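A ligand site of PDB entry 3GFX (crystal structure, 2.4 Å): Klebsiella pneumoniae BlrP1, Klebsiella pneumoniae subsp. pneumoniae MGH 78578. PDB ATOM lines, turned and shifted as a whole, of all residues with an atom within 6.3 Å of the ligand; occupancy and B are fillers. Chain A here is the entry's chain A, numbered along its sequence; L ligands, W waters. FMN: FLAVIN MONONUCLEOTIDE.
Merely in contact with the ligand: Tyr 15 (3.3 Å), Leu 31 (3.8 Å), Arg 34 (3.4 Å), Ala 35 (3.5 Å), Phe 55 (3.8 Å), Leu 59 (3.8 Å), Leu 69 (3.4 Å), Ile 73 (3.4 Å), Arg 78 (3.6 Å), His 79 (3.6 Å) and Met 100 (3.6 Å).
Hydrophobic or aromatic side chains within 4 Å of the ligand: Leu 31, Ala 35, Phe 55, Leu 59, Leu 69, Ile 73, His 79 and Met 100.
Within 4 Å of the ligand: Tyr 15, Leu 31, Arg 34, Ala 35, Lys 38, Asn 39, Phe 55, Gln 57, Leu 59, Leu 69, Glu 72, Ile 73, Asp 76, Arg 78, His 79 and Met 100.
The nearest printed residue that does not touch the ligand is Leu 48 (4.2 Å).
The side-chain carboxylate (OD2) of Asp 76 lies within salt-bridge range of the guanidinium group (NH1) of Arg 78.
The side-chain amino group (NZ) of Lys 38 lies within salt-bridge range of the side-chain carboxylate (OE1) of Glu 72 (3.4 Å).
The backbone carbonyl oxygen (O) of Ala 35 sits close to the side-chain amide oxygen (OD1) of Asn 39 (3.2 Å).
The side-chain amide oxygen (OE1) of Gln 57 is in hydrogen-bond range of the side-chain hydroxyl (OH) of Tyr 15 (2.7 Å).
The side-chain amide nitrogen (NE2) of Gln 57 is in hydrogen-bond range of the side-chain sulfur (SD) of Met 100, at 3.3 Å.
N of Leu 48 is in hydrogen-bond range of SD of Met 100.
The side-chain hydroxyl of Ser 17 lies within hydrogen-bond range of a ring nitrogen (ND1) of His 79 (2.9 Å).
The backbone carbonyl oxygen (O) of Phe 55 is in hydrogen-bond range of the backbone NH (N) of Ser 17, at 3.0 Å.
The side-chain carboxylate of Asp 76 lies within hydrogen-bond range of an oxygen (O2') of the ligand (2.6 Å).
The side-chain amino group (NZ) of Lys 38 lies within salt-bridge range of an oxygen (O2P) of the ligand.
A nitrogen (N3) of the ligand sits at hydrogen-bond distance from the side-chain amide oxygen of Asn 39, at 2.8 Å.
NE2 of Gln 57 lies within hydrogen-bond range of N5 of the ligand (3.1 Å).
The backbone carbonyl oxygen (O) of Glu 72 sits at hydrogen-bond distance from an oxygen (O2') of the ligand (3.5 Å).
Water W6 bridges the side-chain amide oxygen of Asn 39 (2.8 Å) and an oxygen (O2) of the ligand (2.9 Å).
Water W1 lies within hydrogen-bond range of O3' of the ligand and OD2 of Asp 76.
Water W2 lies within hydrogen-bond range of NH2 of Arg 78 (3.0 Å) and O3P of the ligand (3.2 Å).
Water W5 bridges the backbone carbonyl oxygen of Leu 31 and a nitrogen (N1) of the ligand.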
ATOM      1  N   TYR A  15     -25.682   9.152  14.711  1.00  0.00           N
ATOM      2  CA  TYR A  15     -25.753  10.503  14.174  1.00  0.00           C
ATOM      3  C   TYR A  15     -25.905  10.520  12.652  1.00  0.00           C
ATOM      4  O   TYR A  15     -25.700   9.502  11.985  1.00  0.00           O
ATOM      5  CB  TYR A  15     -24.530  11.331  14.592  1.00  0.00           C
ATOM      6  CG  TYR A  15     -23.249  10.974  13.852  1.00  0.00           C
ATOM      7  CD1 TYR A  15     -22.929  11.565  12.637  1.00  0.00           C
ATOM      8  CD2 TYR A  15     -22.354  10.041  14.394  1.00  0.00           C
ATOM      9  CE1 TYR A  15     -21.769  11.235  11.957  1.00  0.00           C
ATOM     10  CE2 TYR A  15     -21.189   9.716  13.726  1.00  0.00           C
ATOM     11  CZ  TYR A  15     -20.901  10.312  12.506  1.00  0.00           C
ATOM     12  OH  TYR A  15     -19.754   9.981  11.832  1.00  0.00           O
ATOM     13  N   SER A  17     -24.846  13.282   9.209  1.00  0.00           N
ATOM     14  CA  SER A  17     -24.115  14.481   8.801  1.00  0.00           C
ATOM     15  C   SER A  17     -24.220  14.737   7.300  1.00  0.00           C
ATOM     16  O   SER A  17     -24.882  13.979   6.590  1.00  0.00           O
ATOM     17  CB  SER A  17     -22.648  14.402   9.225  1.00  0.00           C
ATOM     18  OG  SER A  17     -21.971  13.357   8.538  1.00  0.00           O
ATOM     19  N   LEU A  28     -13.163   7.584   1.017  1.00  0.00           N
ATOM     20  CA  LEU A  28     -13.929   6.895   2.048  1.00  0.00           C
ATOM     21  C   LEU A  28     -13.354   5.508   2.320  1.00  0.00           C
ATOM     22  O   LEU A  28     -13.509   4.971   3.414  1.00  0.00           O
ATOM     23  CB  LEU A  28     -15.397   6.799   1.641  1.00  0.00           C
ATOM     24  CG  LEU A  28     -16.124   8.131   1.543  1.00  0.00           C
ATOM     25  CD1 LEU A  28     -17.518   7.937   1.016  1.00  0.00           C
ATOM     26  CD2 LEU A  28     -16.132   8.843   2.888  1.00  0.00           C
ATOM     27  N   LEU A  31     -10.777   6.216   4.840  1.00  0.00           N
ATOM     28  CA  LEU A  31     -11.468   6.656   6.055  1.00  0.00           C
ATOM     29  C   LEU A  31     -11.952   5.460   6.877  1.00  0.00           C
ATOM     30  O   LEU A  31     -11.568   5.297   8.026  1.00  0.00           O
ATOM     31  CB  LEU A  31     -12.636   7.578   5.707  1.00  0.00           C
ATOM     32  CG  LEU A  31     -13.351   8.390   6.800  1.00  0.00           C
ATOM     33  CD1 LEU A  31     -13.926   9.647   6.200  1.00  0.00           C
ATOM     34  CD2 LEU A  31     -14.463   7.594   7.492  1.00  0.00           C
ATOM     35  N   ARG A  34      -9.135   2.809   8.121  1.00  0.00           N
ATOM     36  CA  ARG A  34      -8.467   3.338   9.292  1.00  0.00           C
ATOM     37  C   ARG A  34      -9.412   3.354  10.499  1.00  0.00           C
ATOM     38  O   ARG A  34      -8.978   3.092  11.620  1.00  0.00           O
ATOM     39  CB  ARG A  34      -7.992   4.762   8.981  1.00  0.00           C
ATOM     40  CG  ARG A  34      -7.218   5.460  10.072  1.00  0.00           C
ATOM     41  CD  ARG A  34      -6.798   6.846   9.587  1.00  0.00           C
ATOM     42  NE  ARG A  34      -6.044   6.777   8.338  1.00  0.00           N
ATOM     43  CZ  ARG A  34      -4.719   6.670   8.268  1.00  0.00           C
ATOM     44  NH1 ARG A  34      -3.985   6.618   9.378  1.00  0.00           N
ATOM     45  NH2 ARG A  34      -4.115   6.614   7.081  1.00  0.00           N
ATOM     46  N   ALA A  35     -10.674   3.695  10.244  1.00  0.00           N
ATOM     47  CA  ALA A  35     -11.704   3.700  11.277  1.00  0.00           C
ATOM     48  C   ALA A  35     -11.870   2.309  11.884  1.00  0.00           C
ATOM     49  O   ALA A  35     -11.794   2.160  13.100  1.00  0.00           O
ATOM     50  CB  ALA A  35     -13.025   4.202  10.717  1.00  0.00           C
ATOM     51  N   SER A  36     -12.061   1.315  11.022  1.00  0.00           N
ATOM     52  CA  SER A  36     -12.242  -0.082  11.441  1.00  0.00           C
ATOM     53  C   SER A  36     -11.024  -0.620  12.180  1.00  0.00           C
ATOM     54  O   SER A  36     -11.160  -1.370  13.151  1.00  0.00           O
ATOM     55  CB  SER A  36     -12.541  -0.952  10.226  1.00  0.00           C
ATOM     56  OG  SER A  36     -12.771  -2.299  10.595  1.00  0.00           O
ATOM     57  N   LYS A  38      -8.908   1.215  13.872  1.00  0.00           N
ATOM     58  CA  LYS A  38      -8.774   1.938  15.132  1.00  0.00           C
ATOM     59  C   LYS A  38      -9.880   1.546  16.108  1.00  0.00           C
ATOM     60  O   LYS A  38      -9.635   1.448  17.309  1.00  0.00           O
ATOM     61  CB  LYS A  38      -8.797   3.456  14.889  1.00  0.00           C
ATOM     62  CG  LYS A  38      -8.330   4.293  16.068  1.00  0.00           C
ATOM     63  CD  LYS A  38      -8.442   5.784  15.757  1.00  0.00           C
ATOM     64  CE  LYS A  38      -8.060   6.626  16.951  1.00  0.00           C
ATOM     65  NZ  LYS A  38      -8.388   8.071  16.745  1.00  0.00           N
ATOM     66  N   ASN A  39     -11.075   1.317  15.584  1.00  0.00           N
ATOM     67  CA  ASN A  39     -12.247   0.995  16.393  1.00  0.00           C
ATOM     68  C   ASN A  39     -12.167  -0.330  17.145  1.00  0.00           C
ATOM     69  O   ASN A  39     -12.487  -0.382  18.338  1.00  0.00           O
ATOM     70  CB  ASN A  39     -13.526   1.010  15.539  1.00  0.00           C
ATOM     71  CG  ASN A  39     -13.990   2.410  15.202  1.00  0.00           C
ATOM     72  OD1 ASN A  39     -13.365   3.399  15.585  1.00  0.00           O
ATOM     73  ND2 ASN A  39     -15.085   2.505  14.469  1.00  0.00           N
ATOM     74  N   ILE A  44     -14.895  -0.770  19.770  1.00  0.00           N
ATOM     75  CA  ILE A  44     -15.912   0.008  19.056  1.00  0.00           C
ATOM     76  C   ILE A  44     -16.340  -0.718  17.782  1.00  0.00           C
ATOM     77  O   ILE A  44     -15.504  -1.190  17.013  1.00  0.00           O
ATOM     78  CB  ILE A  44     -15.409   1.439  18.723  1.00  0.00           C
ATOM     79  CG1 ILE A  44     -14.931   2.158  19.987  1.00  0.00           C
ATOM     80  CG2 ILE A  44     -16.506   2.252  18.017  1.00  0.00           C
ATOM     81  CD1 ILE A  44     -14.224   3.473  19.729  1.00  0.00           C
ATOM     82  N   LEU A  48     -21.366   2.548   8.563  1.00  0.00           N
ATOM     83  CA  LEU A  48     -21.515   3.866   7.965  1.00  0.00           C
ATOM     84  C   LEU A  48     -22.343   3.787   6.677  1.00  0.00           C
ATOM     85  O   LEU A  48     -22.060   2.983   5.800  1.00  0.00           O
ATOM     86  CB  LEU A  48     -20.139   4.486   7.691  1.00  0.00           C
ATOM     87  CG  LEU A  48     -20.063   5.911   7.122  1.00  0.00           C
ATOM     88  CD1 LEU A  48     -20.672   6.934   8.077  1.00  0.00           C
ATOM     89  CD2 LEU A  48     -18.621   6.278   6.806  1.00  0.00           C
ATOM     90  N   PHE A  55     -24.006  11.343   5.494  1.00  0.00           N
ATOM     91  CA  PHE A  55     -23.500  10.206   6.243  1.00  0.00           C
ATOM     92  C   PHE A  55     -24.480   9.824   7.346  1.00  0.00           C
ATOM     93  O   PHE A  55     -25.219  10.667   7.856  1.00  0.00           O
ATOM     94  CB  PHE A  55     -22.134  10.508   6.874  1.00  0.00           C
ATOM     95  CG  PHE A  55     -21.011  10.586   5.883  1.00  0.00           C
ATOM     96  CD1 PHE A  55     -20.550   9.444   5.249  1.00  0.00           C
ATOM     97  CD2 PHE A  55     -20.397  11.800   5.622  1.00  0.00           C
ATOM     98  CE1 PHE A  55     -19.492   9.511   4.345  1.00  0.00           C
ATOM     99  CE2 PHE A  55     -19.354  11.877   4.720  1.00  0.00           C
ATOM    100  CZ  PHE A  55     -18.903  10.742   4.078  1.00  0.00           C
ATOM    101  N   GLN A  57     -24.097   7.181  10.764  1.00  0.00           N
ATOM    102  CA  GLN A  57     -23.213   6.262  11.468  1.00  0.00           C
ATOM    103  C   GLN A  57     -23.776   5.758  12.783  1.00  0.00           C
ATOM    104  O   GLN A  57     -24.263   6.536  13.605  1.00  0.00           O
ATOM    105  CB  GLN A  57     -21.829   6.887  11.679  1.00  0.00           C
ATOM    106  CG  GLN A  57     -20.742   5.884  12.012  1.00  0.00           C
ATOM    107  CD  GLN A  57     -19.360   6.480  11.967  1.00  0.00           C
ATOM    108  OE1 GLN A  57     -19.079   7.495  12.614  1.00  0.00           O
ATOM    109  NE2 GLN A  57     -18.475   5.857  11.208  1.00  0.00           N
ATOM    110  N   LEU A  59     -22.552   3.843  16.168  1.00  0.00           N
ATOM    111  CA  LEU A  59     -21.356   3.522  16.948  1.00  0.00           C
ATOM    112  C   LEU A  59     -21.734   2.757  18.209  1.00  0.00           C
ATOM    113  O   LEU A  59     -22.641   3.150  18.933  1.00  0.00           O
ATOM    114  CB  LEU A  59     -20.598   4.804  17.319  1.00  0.00           C
ATOM    115  CG  LEU A  59     -19.913   5.588  16.198  1.00  0.00           C
ATOM    116  CD1 LEU A  59     -19.442   6.944  16.708  1.00  0.00           C
ATOM    117  CD2 LEU A  59     -18.748   4.798  15.611  1.00  0.00           C
ATOM    118  N   LEU A  69     -14.556   9.321  20.774  1.00  0.00           N
ATOM    119  CA  LEU A  69     -14.604   9.185  19.324  1.00  0.00           C
ATOM    120  C   LEU A  69     -15.469  10.235  18.648  1.00  0.00           C
ATOM    121  O   LEU A  69     -15.032  10.899  17.707  1.00  0.00           O
ATOM    122  CB  LEU A  69     -15.061   7.776  18.928  1.00  0.00           C
ATOM    123  CG  LEU A  69     -15.033   7.457  17.419  1.00  0.00           C
ATOM    124  CD1 LEU A  69     -13.636   7.696  16.856  1.00  0.00           C
ATOM    125  CD2 LEU A  69     -15.497   6.042  17.158  1.00  0.00           C
ATOM    126  N   GLU A  72     -13.987  13.636  18.278  1.00  0.00           N
ATOM    127  CA  GLU A  72     -13.073  13.749  17.143  1.00  0.00           C
ATOM    128  C   GLU A  72     -13.847  13.863  15.835  1.00  0.00           C
ATOM    129  O   GLU A  72     -13.444  14.599  14.927  1.00  0.00           O
ATOM    130  CB  GLU A  72     -12.137  12.537  17.077  1.00  0.00           C
ATOM    131  CG  GLU A  72     -11.036  12.517  18.134  1.00  0.00           C
ATOM    132  CD  GLU A  72     -10.288  11.198  18.171  1.00  0.00           C
ATOM    133  OE1 GLU A  72      -9.078  11.176  17.848  1.00  0.00           O
ATOM    134  OE2 GLU A  72     -10.917  10.160  18.511  1.00  0.00           O
ATOM    135  N   ILE A  73     -14.963  13.138  15.748  1.00  0.00           N
ATOM    136  CA  ILE A  73     -15.816  13.116  14.568  1.00  0.00           C
ATOM    137  C   ILE A  73     -16.518  14.459  14.341  1.00  0.00           C
ATOM    138  O   ILE A  73     -16.607  14.935  13.206  1.00  0.00           O
ATOM    139  CB  ILE A  73     -16.848  11.955  14.638  1.00  0.00           C
ATOM    140  CG1 ILE A  73     -16.147  10.601  14.479  1.00  0.00           C
ATOM    141  CG2 ILE A  73     -17.937  12.110  13.593  1.00  0.00           C
ATOM    142  CD1 ILE A  73     -17.027   9.399  14.759  1.00  0.00           C
ATOM    143  N   GLN A  74     -17.003  15.071  15.419  1.00  0.00           N
ATOM    144  CA  GLN A  74     -17.656  16.380  15.374  1.00  0.00           C
ATOM    145  C   GLN A  74     -16.742  17.496  14.872  1.00  0.00           C
ATOM    146  O   GLN A  74     -17.203  18.451  14.255  1.00  0.00           O
ATOM    147  CB  GLN A  74     -18.195  16.754  16.761  1.00  0.00           C
ATOM    148  CG  GLN A  74     -19.522  16.118  17.120  1.00  0.00           C
ATOM    149  CD  GLN A  74     -19.959  16.441  18.536  1.00  0.00           C
ATOM    150  OE1 GLN A  74     -19.295  16.083  19.508  1.00  0.00           O
ATOM    151  NE2 GLN A  74     -21.093  17.133  18.662  1.00  0.00           N
ATOM    152  N   SER A  75     -15.446  17.360  15.151  1.00  0.00           N
ATOM    153  CA  SER A  75     -14.447  18.353  14.748  1.00  0.00           C
ATOM    154  C   SER A  75     -13.839  18.060  13.382  1.00  0.00           C
ATOM    155  O   SER A  75     -12.985  18.811  12.902  1.00  0.00           O
ATOM    156  CB  SER A  75     -13.331  18.442  15.804  1.00  0.00           C
ATOM    157  OG  SER A  75     -13.793  19.072  16.979  1.00  0.00           O
ATOM    158  N   ASP A  76     -14.261  16.960  12.761  1.00  0.00           N
ATOM    159  CA  ASP A  76     -13.713  16.528  11.476  1.00  0.00           C
ATOM    160  C   ASP A  76     -14.202  17.416  10.327  1.00  0.00           C
ATOM    161  O   ASP A  76     -15.406  17.542  10.106  1.00  0.00           O
ATOM    162  CB  ASP A  76     -14.072  15.062  11.212  1.00  0.00           C
ATOM    163  CG  ASP A  76     -13.122  14.400  10.232  1.00  0.00           C
ATOM    164  OD1 ASP A  76     -12.944  14.922   9.119  1.00  0.00           O
ATOM    165  OD2 ASP A  76     -12.556  13.338  10.575  1.00  0.00           O
ATOM    166  N   ARG A  78     -14.077  16.920   7.197  1.00  0.00           N
ATOM    167  CA  ARG A  78     -14.575  16.170   6.035  1.00  0.00           C
ATOM    168  C   ARG A  78     -16.091  16.270   5.891  1.00  0.00           C
ATOM    169  O   ARG A  78     -16.618  16.128   4.788  1.00  0.00           O
ATOM    170  CB  ARG A  78     -14.159  14.703   6.117  1.00  0.00           C
ATOM    171  CG  ARG A  78     -12.666  14.427   6.050  1.00  0.00           C
ATOM    172  CD  ARG A  78     -12.466  12.933   6.026  1.00  0.00           C
ATOM    173  NE  ARG A  78     -11.121  12.494   6.395  1.00  0.00           N
ATOM    174  CZ  ARG A  78     -10.814  11.902   7.542  1.00  0.00           C
ATOM    175  NH1 ARG A  78     -11.759  11.685   8.463  1.00  0.00           N
ATOM    176  NH2 ARG A  78      -9.570  11.522   7.788  1.00  0.00           N
ATOM    177  N   HIS A  79     -16.776  16.481   7.004  1.00  0.00           N
ATOM    178  CA  HIS A  79     -18.225  16.670   6.992  1.00  0.00           C
ATOM    179  C   HIS A  79     -18.698  17.833   7.867  1.00  0.00           C
ATOM    180  O   HIS A  79     -17.917  18.413   8.629  1.00  0.00           O
ATOM    181  CB  HIS A  79     -18.966  15.368   7.357  1.00  0.00           C
ATOM    182  CG  HIS A  79     -18.730  14.876   8.750  1.00  0.00           C
ATOM    183  ND1 HIS A  79     -19.209  13.673   9.199  1.00  0.00           N
ATOM    184  CD2 HIS A  79     -18.055  15.428   9.802  1.00  0.00           C
ATOM    185  CE1 HIS A  79     -18.865  13.493  10.460  1.00  0.00           C
ATOM    186  NE2 HIS A  79     -18.155  14.537  10.844  1.00  0.00           N
ATOM    187  N   GLY A  99     -15.590  -3.378  13.149  1.00  0.00           N
ATOM    188  CA  GLY A  99     -15.100  -2.118  13.709  1.00  0.00           C
ATOM    189  C   GLY A  99     -15.716  -0.918  13.026  1.00  0.00           C
ATOM    190  O   GLY A  99     -16.227  -0.005  13.670  1.00  0.00           O
ATOM    191  N   MET A 100     -15.665  -0.934  11.690  1.00  0.00           N
ATOM    192  CA  MET A 100     -16.374   0.034  10.848  1.00  0.00           C
ATOM    193  C   MET A 100     -16.502  -0.531   9.430  1.00  0.00           C
ATOM    194  O   MET A 100     -15.625  -1.254   8.961  1.00  0.00           O
ATOM    195  CB  MET A 100     -15.653   1.387  10.837  1.00  0.00           C
ATOM    196  CG  MET A 100     -16.467   2.562  10.251  1.00  0.00           C
ATOM    197  SD  MET A 100     -18.230   2.579  10.656  1.00  0.00           S
ATOM    198  CE  MET A 100     -18.220   2.718  12.454  1.00  0.00           C
HETATM  199  N1  FMN L   1     -12.582   7.576  13.071  1.00  0.00           N
HETATM  200  C2  FMN L   1     -12.602   6.424  13.838  1.00  0.00           C
HETATM  201  O2  FMN L   1     -11.611   6.111  14.483  1.00  0.00           O
HETATM  202  N3  FMN L   1     -13.734   5.649  13.884  1.00  0.00           N
HETATM  203  C4  FMN L   1     -14.857   5.998  13.153  1.00  0.00           C
HETATM  204  O4  FMN L   1     -15.852   5.278  13.179  1.00  0.00           O
HETATM  205  C4A FMN L   1     -14.835   7.157  12.374  1.00  0.00           C
HETATM  206  N5  FMN L   1     -15.954   7.521  11.653  1.00  0.00           N
HETATM  207  C5A FMN L   1     -15.951   8.658  10.882  1.00  0.00           C
HETATM  208  C6  FMN L   1     -17.088   9.008  10.157  1.00  0.00           C
HETATM  209  C7  FMN L   1     -17.101  10.156   9.364  1.00  0.00           C
HETATM  210  C7M FMN L   1     -18.159  10.265   8.300  1.00  0.00           C
HETATM  211  C8  FMN L   1     -15.955  10.964   9.315  1.00  0.00           C
HETATM  212  C8M FMN L   1     -15.969  12.255   8.559  1.00  0.00           C
HETATM  213  C9  FMN L   1     -14.823  10.617  10.048  1.00  0.00           C
HETATM  214  C9A FMN L   1     -14.805   9.466  10.833  1.00  0.00           C
HETATM  215  N10 FMN L   1     -13.681   9.107  11.567  1.00  0.00           N
HETATM  216  C10 FMN L   1     -13.701   7.956  12.334  1.00  0.00           C
HETATM  217  C1' FMN L   1     -12.456   9.991  11.545  1.00  0.00           C
HETATM  218  C2' FMN L   1     -12.340  10.843  12.815  1.00  0.00           C
HETATM  219  O2' FMN L   1     -13.172  11.974  12.703  1.00  0.00           O
HETATM  220  C3' FMN L   1     -10.910  11.303  13.085  1.00  0.00           C
HETATM  221  O3' FMN L   1     -10.320  11.804  11.900  1.00  0.00           O
HETATM  222  C4' FMN L   1     -10.015  10.202  13.665  1.00  0.00           C
HETATM  223  O4' FMN L   1     -10.660   9.544  14.734  1.00  0.00           O
HETATM  224  C5' FMN L   1      -8.691  10.778  14.149  1.00  0.00           C
HETATM  225  O5' FMN L   1      -7.845   9.752  14.603  1.00  0.00           O
HETATM  226  P   FMN L   1      -6.540   9.313  13.772  1.00  0.00           P
HETATM  227  O1P FMN L   1      -5.691  10.544  13.525  1.00  0.00           O
HETATM  228  O2P FMN L   1      -5.755   8.297  14.573  1.00  0.00           O
HETATM  229  O3P FMN L   1      -6.949   8.710  12.449  1.00  0.00           O
HETATM  230  O   HOH W   1      -9.863  14.624  11.363  1.00  0.00           O
HETATM  231  O   HOH W   2      -8.692   9.662   9.949  1.00  0.00           O
HETATM  232  O   HOH W   3      -5.761  10.025  10.229  1.00  0.00           O
HETATM  233  O   HOH W   4      -9.671   6.665  12.480  1.00  0.00           O
HETATM  234  O   HOH W   5     -11.072   7.207  10.139  1.00  0.00           O
HETATM  235  O   HOH W   6     -11.597   4.906  17.070  1.00  0.00           O
